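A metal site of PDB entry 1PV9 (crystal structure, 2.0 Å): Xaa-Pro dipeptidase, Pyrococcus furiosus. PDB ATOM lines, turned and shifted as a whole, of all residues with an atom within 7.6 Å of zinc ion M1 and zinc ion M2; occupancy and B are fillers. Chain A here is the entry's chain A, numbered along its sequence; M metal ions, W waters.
Zinc ion M2 is bound by OE1 of Glu 327, OD1 of Asp 220, OD1 of Asp 209 and water W1.
Slightly farther from zinc ion M2 lies the side-chain carboxylate (OD2) of Asp 209 (2.8 Å).
Residues that only touch zinc ion M2: Thr 222 (3.4 Å) and Phe 178 (3.8 Å).
Zinc ion M1 is bound by water W1, OE2 of Glu 327, NE2 of His 284, OD2 of Asp 220 and OE2 of Glu 313.
Zinc ion M1 has five donor atoms within binding distance.
The backbone carbonyl oxygen (O) of Thr 222 is in hydrogen-bond range of the backbone NH (N) of Glu 327 (2.9 Å).
The guanidinium group (NH2) of Arg 325 lies within salt-bridge range of the side-chain carboxylate (OD2) of Asp 209 (2.8 Å).
O of Ile 290 lies close to ND1 of His 284.
O of Asp 220 is in hydrogen-bond range of OG1 of Thr 329 (2.7 Å).
The backbone carbonyl oxygen (O) of His 284 lies within hydrogen-bond range of the backbone NH (N) of Thr 311 (2.8 Å).
The side-chain carboxylate of Glu 313 sits close to the side-chain hydroxyl of Thr 311.
O of Asp 209 lies within hydrogen-bond range of N of Ile 181 (2.8 Å).
OG1 of Thr 222 sits close to OD2 of Asp 209, 2.9 Å away.
Merely in contact with zinc ion M1: Thr 311 (3.8 Å).
Of the 27 residues printed, 5 come within 4 Å of zinc ion M1.
Water W1 lies within hydrogen-bond range of OE1 of Glu 313 (3.0 Å) and OD2 of Asp 209 (3.4 Å).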
ATOM      1  N   PHE A 178     -13.459  10.579 -27.293  1.00  0.00           N
ATOM      2  CA  PHE A 178     -13.028  11.935 -27.587  1.00  0.00           C
ATOM      3  C   PHE A 178     -11.565  11.900 -28.006  1.00  0.00           C
ATOM      4  O   PHE A 178     -10.887  10.878 -27.821  1.00  0.00           O
ATOM      5  CB  PHE A 178     -13.227  12.863 -26.366  1.00  0.00           C
ATOM      6  CG  PHE A 178     -12.538  12.381 -25.123  1.00  0.00           C
ATOM      7  CD1 PHE A 178     -11.244  12.795 -24.809  1.00  0.00           C
ATOM      8  CD2 PHE A 178     -13.189  11.510 -24.241  1.00  0.00           C
ATOM      9  CE1 PHE A 178     -10.613  12.351 -23.650  1.00  0.00           C
ATOM     10  CE2 PHE A 178     -12.562  11.059 -23.086  1.00  0.00           C
ATOM     11  CZ  PHE A 178     -11.277  11.475 -22.793  1.00  0.00           C
ATOM     12  N   ILE A 181      -5.990  12.703 -25.141  1.00  0.00           N
ATOM     13  CA  ILE A 181      -5.038  13.664 -24.615  1.00  0.00           C
ATOM     14  C   ILE A 181      -3.795  12.932 -24.120  1.00  0.00           C
ATOM     15  O   ILE A 181      -3.859  12.124 -23.196  1.00  0.00           O
ATOM     16  CB  ILE A 181      -5.688  14.517 -23.492  1.00  0.00           C
ATOM     17  CG1 ILE A 181      -6.711  15.505 -24.079  1.00  0.00           C
ATOM     18  CG2 ILE A 181      -4.626  15.270 -22.675  1.00  0.00           C
ATOM     19  CD1 ILE A 181      -7.902  15.756 -23.185  1.00  0.00           C
ATOM     20  N   PRO A 191      -5.298  21.536 -19.779  1.00  0.00           N
ATOM     21  CA  PRO A 191      -6.301  20.484 -19.502  1.00  0.00           C
ATOM     22  C   PRO A 191      -6.753  19.723 -20.747  1.00  0.00           C
ATOM     23  O   PRO A 191      -6.926  18.504 -20.680  1.00  0.00           O
ATOM     24  CB  PRO A 191      -7.465  21.266 -18.900  1.00  0.00           C
ATOM     25  CG  PRO A 191      -6.823  22.447 -18.255  1.00  0.00           C
ATOM     26  CD  PRO A 191      -5.704  22.829 -19.186  1.00  0.00           C
ATOM     27  N   HIS A 192      -6.949  20.420 -21.863  1.00  0.00           N
ATOM     28  CA  HIS A 192      -7.361  19.778 -23.116  1.00  0.00           C
ATOM     29  C   HIS A 192      -6.211  19.683 -24.122  1.00  0.00           C
ATOM     30  O   HIS A 192      -6.379  19.944 -25.312  1.00  0.00           O
ATOM     31  CB  HIS A 192      -8.579  20.492 -23.721  1.00  0.00           C
ATOM     32  CG  HIS A 192      -9.861  20.251 -22.970  1.00  0.00           C
ATOM     33  ND1 HIS A 192     -10.042  19.175 -22.135  1.00  0.00           N
ATOM     34  CD2 HIS A 192     -11.015  20.951 -22.936  1.00  0.00           C
ATOM     35  CE1 HIS A 192     -11.248  19.218 -21.608  1.00  0.00           C
ATOM     36  NE2 HIS A 192     -11.867  20.292 -22.079  1.00  0.00           N
ATOM     37  N   ILE A 208      -2.484  11.642 -19.343  1.00  0.00           N
ATOM     38  CA  ILE A 208      -3.116  10.711 -20.265  1.00  0.00           C
ATOM     39  C   ILE A 208      -4.618  10.688 -20.002  1.00  0.00           C
ATOM     40  O   ILE A 208      -5.071  10.141 -18.991  1.00  0.00           O
ATOM     41  CB  ILE A 208      -2.520   9.277 -20.130  1.00  0.00           C
ATOM     42  CG1 ILE A 208      -0.996   9.306 -20.300  1.00  0.00           C
ATOM     43  CG2 ILE A 208      -3.144   8.336 -21.155  1.00  0.00           C
ATOM     44  CD1 ILE A 208      -0.264   8.365 -19.359  1.00  0.00           C
ATOM     45  N   ASP A 209      -5.364  11.296 -20.901  1.00  0.00           N
ATOM     46  CA  ASP A 209      -6.818  11.430 -20.767  1.00  0.00           C
ATOM     47  C   ASP A 209      -7.473  10.787 -21.974  1.00  0.00           C
ATOM     48  O   ASP A 209      -7.338  11.278 -23.099  1.00  0.00           O
ATOM     49  CB  ASP A 209      -7.207  12.908 -20.656  1.00  0.00           C
ATOM     50  CG  ASP A 209      -8.599  13.116 -20.102  1.00  0.00           C
ATOM     51  OD1 ASP A 209      -9.442  12.196 -20.177  1.00  0.00           O
ATOM     52  OD2 ASP A 209      -8.959  14.191 -19.552  1.00  0.00           O
ATOM     53  N   LEU A 210      -8.181   9.678 -21.751  1.00  0.00           N
ATOM     54  CA  LEU A 210      -8.805   8.937 -22.846  1.00  0.00           C
ATOM     55  C   LEU A 210     -10.132   8.312 -22.430  1.00  0.00           C
ATOM     56  O   LEU A 210     -10.452   8.217 -21.248  1.00  0.00           O
ATOM     57  CB  LEU A 210      -7.842   7.861 -23.383  1.00  0.00           C
ATOM     58  CG  LEU A 210      -7.306   6.781 -22.440  1.00  0.00           C
ATOM     59  CD1 LEU A 210      -8.273   5.616 -22.307  1.00  0.00           C
ATOM     60  CD2 LEU A 210      -5.939   6.281 -22.914  1.00  0.00           C
ATOM     61  N   GLY A 211     -10.906   7.901 -23.431  1.00  0.00           N
ATOM     62  CA  GLY A 211     -12.143   7.176 -23.210  1.00  0.00           C
ATOM     63  C   GLY A 211     -12.538   6.343 -24.414  1.00  0.00           C
ATOM     64  O   GLY A 211     -12.082   6.589 -25.533  1.00  0.00           O
ATOM     65  N   SER A 219     -16.933   6.087 -21.781  1.00  0.00           N
ATOM     66  CA  SER A 219     -16.087   5.977 -20.596  1.00  0.00           C
ATOM     67  C   SER A 219     -15.101   7.139 -20.582  1.00  0.00           C
ATOM     68  O   SER A 219     -14.891   7.790 -21.603  1.00  0.00           O
ATOM     69  CB  SER A 219     -15.329   4.659 -20.613  1.00  0.00           C
ATOM     70  OG  SER A 219     -14.409   4.620 -21.683  1.00  0.00           O
ATOM     71  N   ASP A 220     -14.492   7.369 -19.422  1.00  0.00           N
ATOM     72  CA  ASP A 220     -13.602   8.519 -19.243  1.00  0.00           C
ATOM     73  C   ASP A 220     -12.607   8.244 -18.113  1.00  0.00           C
ATOM     74  O   ASP A 220     -12.995   7.945 -16.979  1.00  0.00           O
ATOM     75  CB  ASP A 220     -14.434   9.763 -18.926  1.00  0.00           C
ATOM     76  CG  ASP A 220     -13.745  11.053 -19.345  1.00  0.00           C
ATOM     77  OD1 ASP A 220     -12.529  11.046 -19.629  1.00  0.00           O
ATOM     78  OD2 ASP A 220     -14.372  12.139 -19.408  1.00  0.00           O
ATOM     79  N   ILE A 221     -11.314   8.353 -18.426  1.00  0.00           N
ATOM     80  CA  ILE A 221     -10.252   8.112 -17.442  1.00  0.00           C
ATOM     81  C   ILE A 221      -9.031   9.024 -17.679  1.00  0.00           C
ATOM     82  O   ILE A 221      -8.652   9.277 -18.814  1.00  0.00           O
ATOM     83  CB  ILE A 221      -9.837   6.607 -17.421  1.00  0.00           C
ATOM     84  CG1 ILE A 221      -8.869   6.326 -16.266  1.00  0.00           C
ATOM     85  CG2 ILE A 221      -9.264   6.162 -18.782  1.00  0.00           C
ATOM     86  CD1 ILE A 221      -8.557   4.858 -16.062  1.00  0.00           C
ATOM     87  N   THR A 222      -8.448   9.519 -16.581  1.00  0.00           N
ATOM     88  CA  THR A 222      -7.197  10.258 -16.656  1.00  0.00           C
ATOM     89  C   THR A 222      -6.200   9.735 -15.637  1.00  0.00           C
ATOM     90  O   THR A 222      -6.527   9.534 -14.469  1.00  0.00           O
ATOM     91  CB  THR A 222      -7.410  11.775 -16.437  1.00  0.00           C
ATOM     92  OG1 THR A 222      -8.331  12.267 -17.418  1.00  0.00           O
ATOM     93  CG2 THR A 222      -6.132  12.554 -16.752  1.00  0.00           C
ATOM     94  N   LEU A 282     -14.974  19.896 -11.126  1.00  0.00           N
ATOM     95  CA  LEU A 282     -14.546  18.589 -10.602  1.00  0.00           C
ATOM     96  C   LEU A 282     -14.850  17.437 -11.553  1.00  0.00           C
ATOM     97  O   LEU A 282     -14.129  16.450 -11.591  1.00  0.00           O
ATOM     98  CB  LEU A 282     -15.191  18.310  -9.243  1.00  0.00           C
ATOM     99  CG  LEU A 282     -14.420  17.579  -8.116  1.00  0.00           C
ATOM    100  CD1 LEU A 282     -15.331  16.575  -7.404  1.00  0.00           C
ATOM    101  CD2 LEU A 282     -13.128  16.903  -8.574  1.00  0.00           C
ATOM    102  N   GLY A 283     -15.952  17.549 -12.312  1.00  0.00           N
ATOM    103  CA  GLY A 283     -16.347  16.489 -13.215  1.00  0.00           C
ATOM    104  C   GLY A 283     -17.627  16.736 -13.977  1.00  0.00           C
ATOM    105  O   GLY A 283     -18.157  17.847 -13.984  1.00  0.00           O
ATOM    106  N   HIS A 284     -18.133  15.673 -14.601  1.00  0.00           N
ATOM    107  CA  HIS A 284     -19.295  15.754 -15.484  1.00  0.00           C
ATOM    108  C   HIS A 284     -19.984  14.397 -15.564  1.00  0.00           C
ATOM    109  O   HIS A 284     -19.397  13.370 -15.235  1.00  0.00           O
ATOM    110  CB  HIS A 284     -18.868  16.178 -16.892  1.00  0.00           C
ATOM    111  CG  HIS A 284     -17.784  15.322 -17.464  1.00  0.00           C
ATOM    112  ND1 HIS A 284     -18.041  14.152 -18.140  1.00  0.00           N
ATOM    113  CD2 HIS A 284     -16.429  15.447 -17.426  1.00  0.00           C
ATOM    114  CE1 HIS A 284     -16.898  13.595 -18.523  1.00  0.00           C
ATOM    115  NE2 HIS A 284     -15.910  14.369 -18.091  1.00  0.00           N
ATOM    116  N   GLY A 285     -21.240  14.406 -16.013  1.00  0.00           N
ATOM    117  CA  GLY A 285     -21.971  13.182 -16.265  1.00  0.00           C
ATOM    118  C   GLY A 285     -21.460  12.474 -17.499  1.00  0.00           C
ATOM    119  O   GLY A 285     -20.865  13.100 -18.385  1.00  0.00           O
ATOM    120  N   VAL A 286     -21.654  11.164 -17.540  1.00  0.00           N
ATOM    121  CA  VAL A 286     -21.264  10.343 -18.687  1.00  0.00           C
ATOM    122  C   VAL A 286     -22.393   9.373 -19.020  1.00  0.00           C
ATOM    123  O   VAL A 286     -22.980   8.775 -18.119  1.00  0.00           O
ATOM    124  CB  VAL A 286     -19.960   9.529 -18.441  1.00  0.00           C
ATOM    125  CG1 VAL A 286     -19.426   8.968 -19.745  1.00  0.00           C
ATOM    126  CG2 VAL A 286     -18.906  10.379 -17.765  1.00  0.00           C
ATOM    127  N   ILE A 290     -20.149  11.905 -23.969  1.00  0.00           N
ATOM    128  CA  ILE A 290     -18.998  11.967 -23.071  1.00  0.00           C
ATOM    129  C   ILE A 290     -19.181  13.036 -21.981  1.00  0.00           C
ATOM    130  O   ILE A 290     -18.797  12.840 -20.829  1.00  0.00           O
ATOM    131  CB  ILE A 290     -17.661  12.137 -23.862  1.00  0.00           C
ATOM    132  CG1 ILE A 290     -16.441  12.063 -22.939  1.00  0.00           C
ATOM    133  CG2 ILE A 290     -17.644  13.458 -24.651  1.00  0.00           C
ATOM    134  CD1 ILE A 290     -16.224  10.711 -22.284  1.00  0.00           C
ATOM    135  N   HIS A 291     -19.809  14.150 -22.357  1.00  0.00           N
ATOM    136  CA  HIS A 291     -20.132  15.207 -21.401  1.00  0.00           C
ATOM    137  C   HIS A 291     -21.651  15.311 -21.248  1.00  0.00           C
ATOM    138  O   HIS A 291     -22.362  15.637 -22.203  1.00  0.00           O
ATOM    139  CB  HIS A 291     -19.531  16.549 -21.830  1.00  0.00           C
ATOM    140  CG  HIS A 291     -18.078  16.693 -21.471  1.00  0.00           C
ATOM    141  ND1 HIS A 291     -17.604  17.748 -20.727  1.00  0.00           N
ATOM    142  CD2 HIS A 291     -17.012  15.922 -21.753  1.00  0.00           C
ATOM    143  CE1 HIS A 291     -16.299  17.620 -20.570  1.00  0.00           C
ATOM    144  NE2 HIS A 291     -15.910  16.514 -21.180  1.00  0.00           N
ATOM    145  N   ILE A 310     -20.943   9.703 -13.137  1.00  0.00           N
ATOM    146  CA  ILE A 310     -20.189  10.950 -13.193  1.00  0.00           C
ATOM    147  C   ILE A 310     -18.683  10.695 -13.196  1.00  0.00           C
ATOM    148  O   ILE A 310     -18.234   9.586 -12.877  1.00  0.00           O
ATOM    149  CB  ILE A 310     -20.566  11.880 -11.995  1.00  0.00           C
ATOM    150  CG1 ILE A 310     -20.416  11.129 -10.667  1.00  0.00           C
ATOM    151  CG2 ILE A 310     -21.972  12.442 -12.159  1.00  0.00           C
ATOM    152  CD1 ILE A 310     -20.036  12.010  -9.490  1.00  0.00           C
ATOM    153  N   THR A 311     -17.910  11.725 -13.537  1.00  0.00           N
ATOM    154  CA  THR A 311     -16.467  11.681 -13.345  1.00  0.00           C
ATOM    155  C   THR A 311     -16.043  12.539 -12.155  1.00  0.00           C
ATOM    156  O   THR A 311     -16.718  13.495 -11.780  1.00  0.00           O
ATOM    157  CB  THR A 311     -15.712  12.154 -14.611  1.00  0.00           C
ATOM    158  OG1 THR A 311     -16.061  13.510 -14.910  1.00  0.00           O
ATOM    159  CG2 THR A 311     -16.143  11.370 -15.839  1.00  0.00           C
ATOM    160  N   ILE A 312     -14.915  12.165 -11.568  1.00  0.00           N
ATOM    161  CA  ILE A 312     -14.296  12.946 -10.497  1.00  0.00           C
ATOM    162  C   ILE A 312     -12.850  13.153 -10.910  1.00  0.00           C
ATOM    163  O   ILE A 312     -12.057  12.201 -10.906  1.00  0.00           O
ATOM    164  CB  ILE A 312     -14.440  12.221  -9.132  1.00  0.00           C
ATOM    165  CG1 ILE A 312     -15.914  12.243  -8.671  1.00  0.00           C
ATOM    166  CG2 ILE A 312     -13.568  12.886  -8.070  1.00  0.00           C
ATOM    167  CD1 ILE A 312     -16.300  11.122  -7.717  1.00  0.00           C
ATOM    168  N   GLU A 313     -12.524  14.377 -11.298  1.00  0.00           N
ATOM    169  CA  GLU A 313     -11.235  14.652 -11.936  1.00  0.00           C
ATOM    170  C   GLU A 313     -10.636  16.014 -11.565  1.00  0.00           C
ATOM    171  O   GLU A 313     -10.615  16.931 -12.381  1.00  0.00           O
ATOM    172  CB  GLU A 313     -11.353  14.528 -13.457  1.00  0.00           C
ATOM    173  CG  GLU A 313     -12.471  15.328 -14.113  1.00  0.00           C
ATOM    174  CD  GLU A 313     -12.505  15.193 -15.622  1.00  0.00           C
ATOM    175  OE1 GLU A 313     -11.442  15.227 -16.276  1.00  0.00           O
ATOM    176  OE2 GLU A 313     -13.616  15.045 -16.167  1.00  0.00           O
ATOM    177  N   ARG A 325      -3.600  15.657 -13.488  1.00  0.00           N
ATOM    178  CA  ARG A 325      -5.019  15.353 -13.384  1.00  0.00           C
ATOM    179  C   ARG A 325      -5.190  13.856 -13.163  1.00  0.00           C
ATOM    180  O   ARG A 325      -4.483  13.052 -13.774  1.00  0.00           O
ATOM    181  CB  ARG A 325      -5.789  15.813 -14.624  1.00  0.00           C
ATOM    182  CG  ARG A 325      -7.279  15.464 -14.627  1.00  0.00           C
ATOM    183  CD  ARG A 325      -8.120  16.216 -15.669  1.00  0.00           C
ATOM    184  NE  ARG A 325      -7.841  15.794 -17.043  1.00  0.00           N
ATOM    185  CZ  ARG A 325      -7.068  16.467 -17.900  1.00  0.00           C
ATOM    186  NH1 ARG A 325      -6.475  17.592 -17.538  1.00  0.00           N
ATOM    187  NH2 ARG A 325      -6.887  15.990 -19.122  1.00  0.00           N
ATOM    188  N   GLU A 327      -8.484  11.131 -12.987  1.00  0.00           N
ATOM    189  CA  GLU A 327      -9.917  11.030 -13.243  1.00  0.00           C
ATOM    190  C   GLU A 327     -10.428   9.599 -13.201  1.00  0.00           C
ATOM    191  O   GLU A 327      -9.809   8.693 -13.771  1.00  0.00           O
ATOM    192  CB  GLU A 327     -10.271  11.668 -14.587  1.00  0.00           C
ATOM    193  CG  GLU A 327     -11.642  11.300 -15.141  1.00  0.00           C
ATOM    194  CD  GLU A 327     -11.923  11.941 -16.486  1.00  0.00           C
ATOM    195  OE1 GLU A 327     -11.000  11.990 -17.329  1.00  0.00           O
ATOM    196  OE2 GLU A 327     -13.063  12.389 -16.710  1.00  0.00           O
ATOM    197  N   ASP A 328     -11.568   9.422 -12.545  1.00  0.00           N
ATOM    198  CA  ASP A 328     -12.289   8.156 -12.554  1.00  0.00           C
ATOM    199  C   ASP A 328     -13.705   8.330 -13.098  1.00  0.00           C
ATOM    200  O   ASP A 328     -14.294   9.403 -12.964  1.00  0.00           O
ATOM    201  CB  ASP A 328     -12.386   7.580 -11.133  1.00  0.00           C
ATOM    202  CG  ASP A 328     -11.153   6.821 -10.735  1.00  0.00           C
ATOM    203  OD1 ASP A 328     -10.696   5.953 -11.511  1.00  0.00           O
ATOM    204  OD2 ASP A 328     -10.570   7.009  -9.641  1.00  0.00           O
ATOM    205  N   THR A 329     -14.238   7.284 -13.719  1.00  0.00           N
ATOM    206  CA  THR A 329     -15.668   7.224 -13.986  1.00  0.00           C
ATOM    207  C   THR A 329     -16.323   6.523 -12.792  1.00  0.00           C
ATOM    208  O   THR A 329     -15.893   5.431 -12.400  1.00  0.00           O
ATOM    209  CB  THR A 329     -15.963   6.497 -15.312  1.00  0.00           C
ATOM    210  OG1 THR A 329     -15.566   7.336 -16.399  1.00  0.00           O
ATOM    211  CG2 THR A 329     -17.466   6.360 -15.528  1.00  0.00           C
HETATM  212 ZN    ZN M   1     -13.859  13.756 -18.034  1.00  0.00          ZN
HETATM  213 ZN    ZN M   2     -11.250  12.607 -19.200  1.00  0.00          ZN
HETATM  214  O   HOH W   1     -12.264  14.450 -19.048  1.00  0.00           O
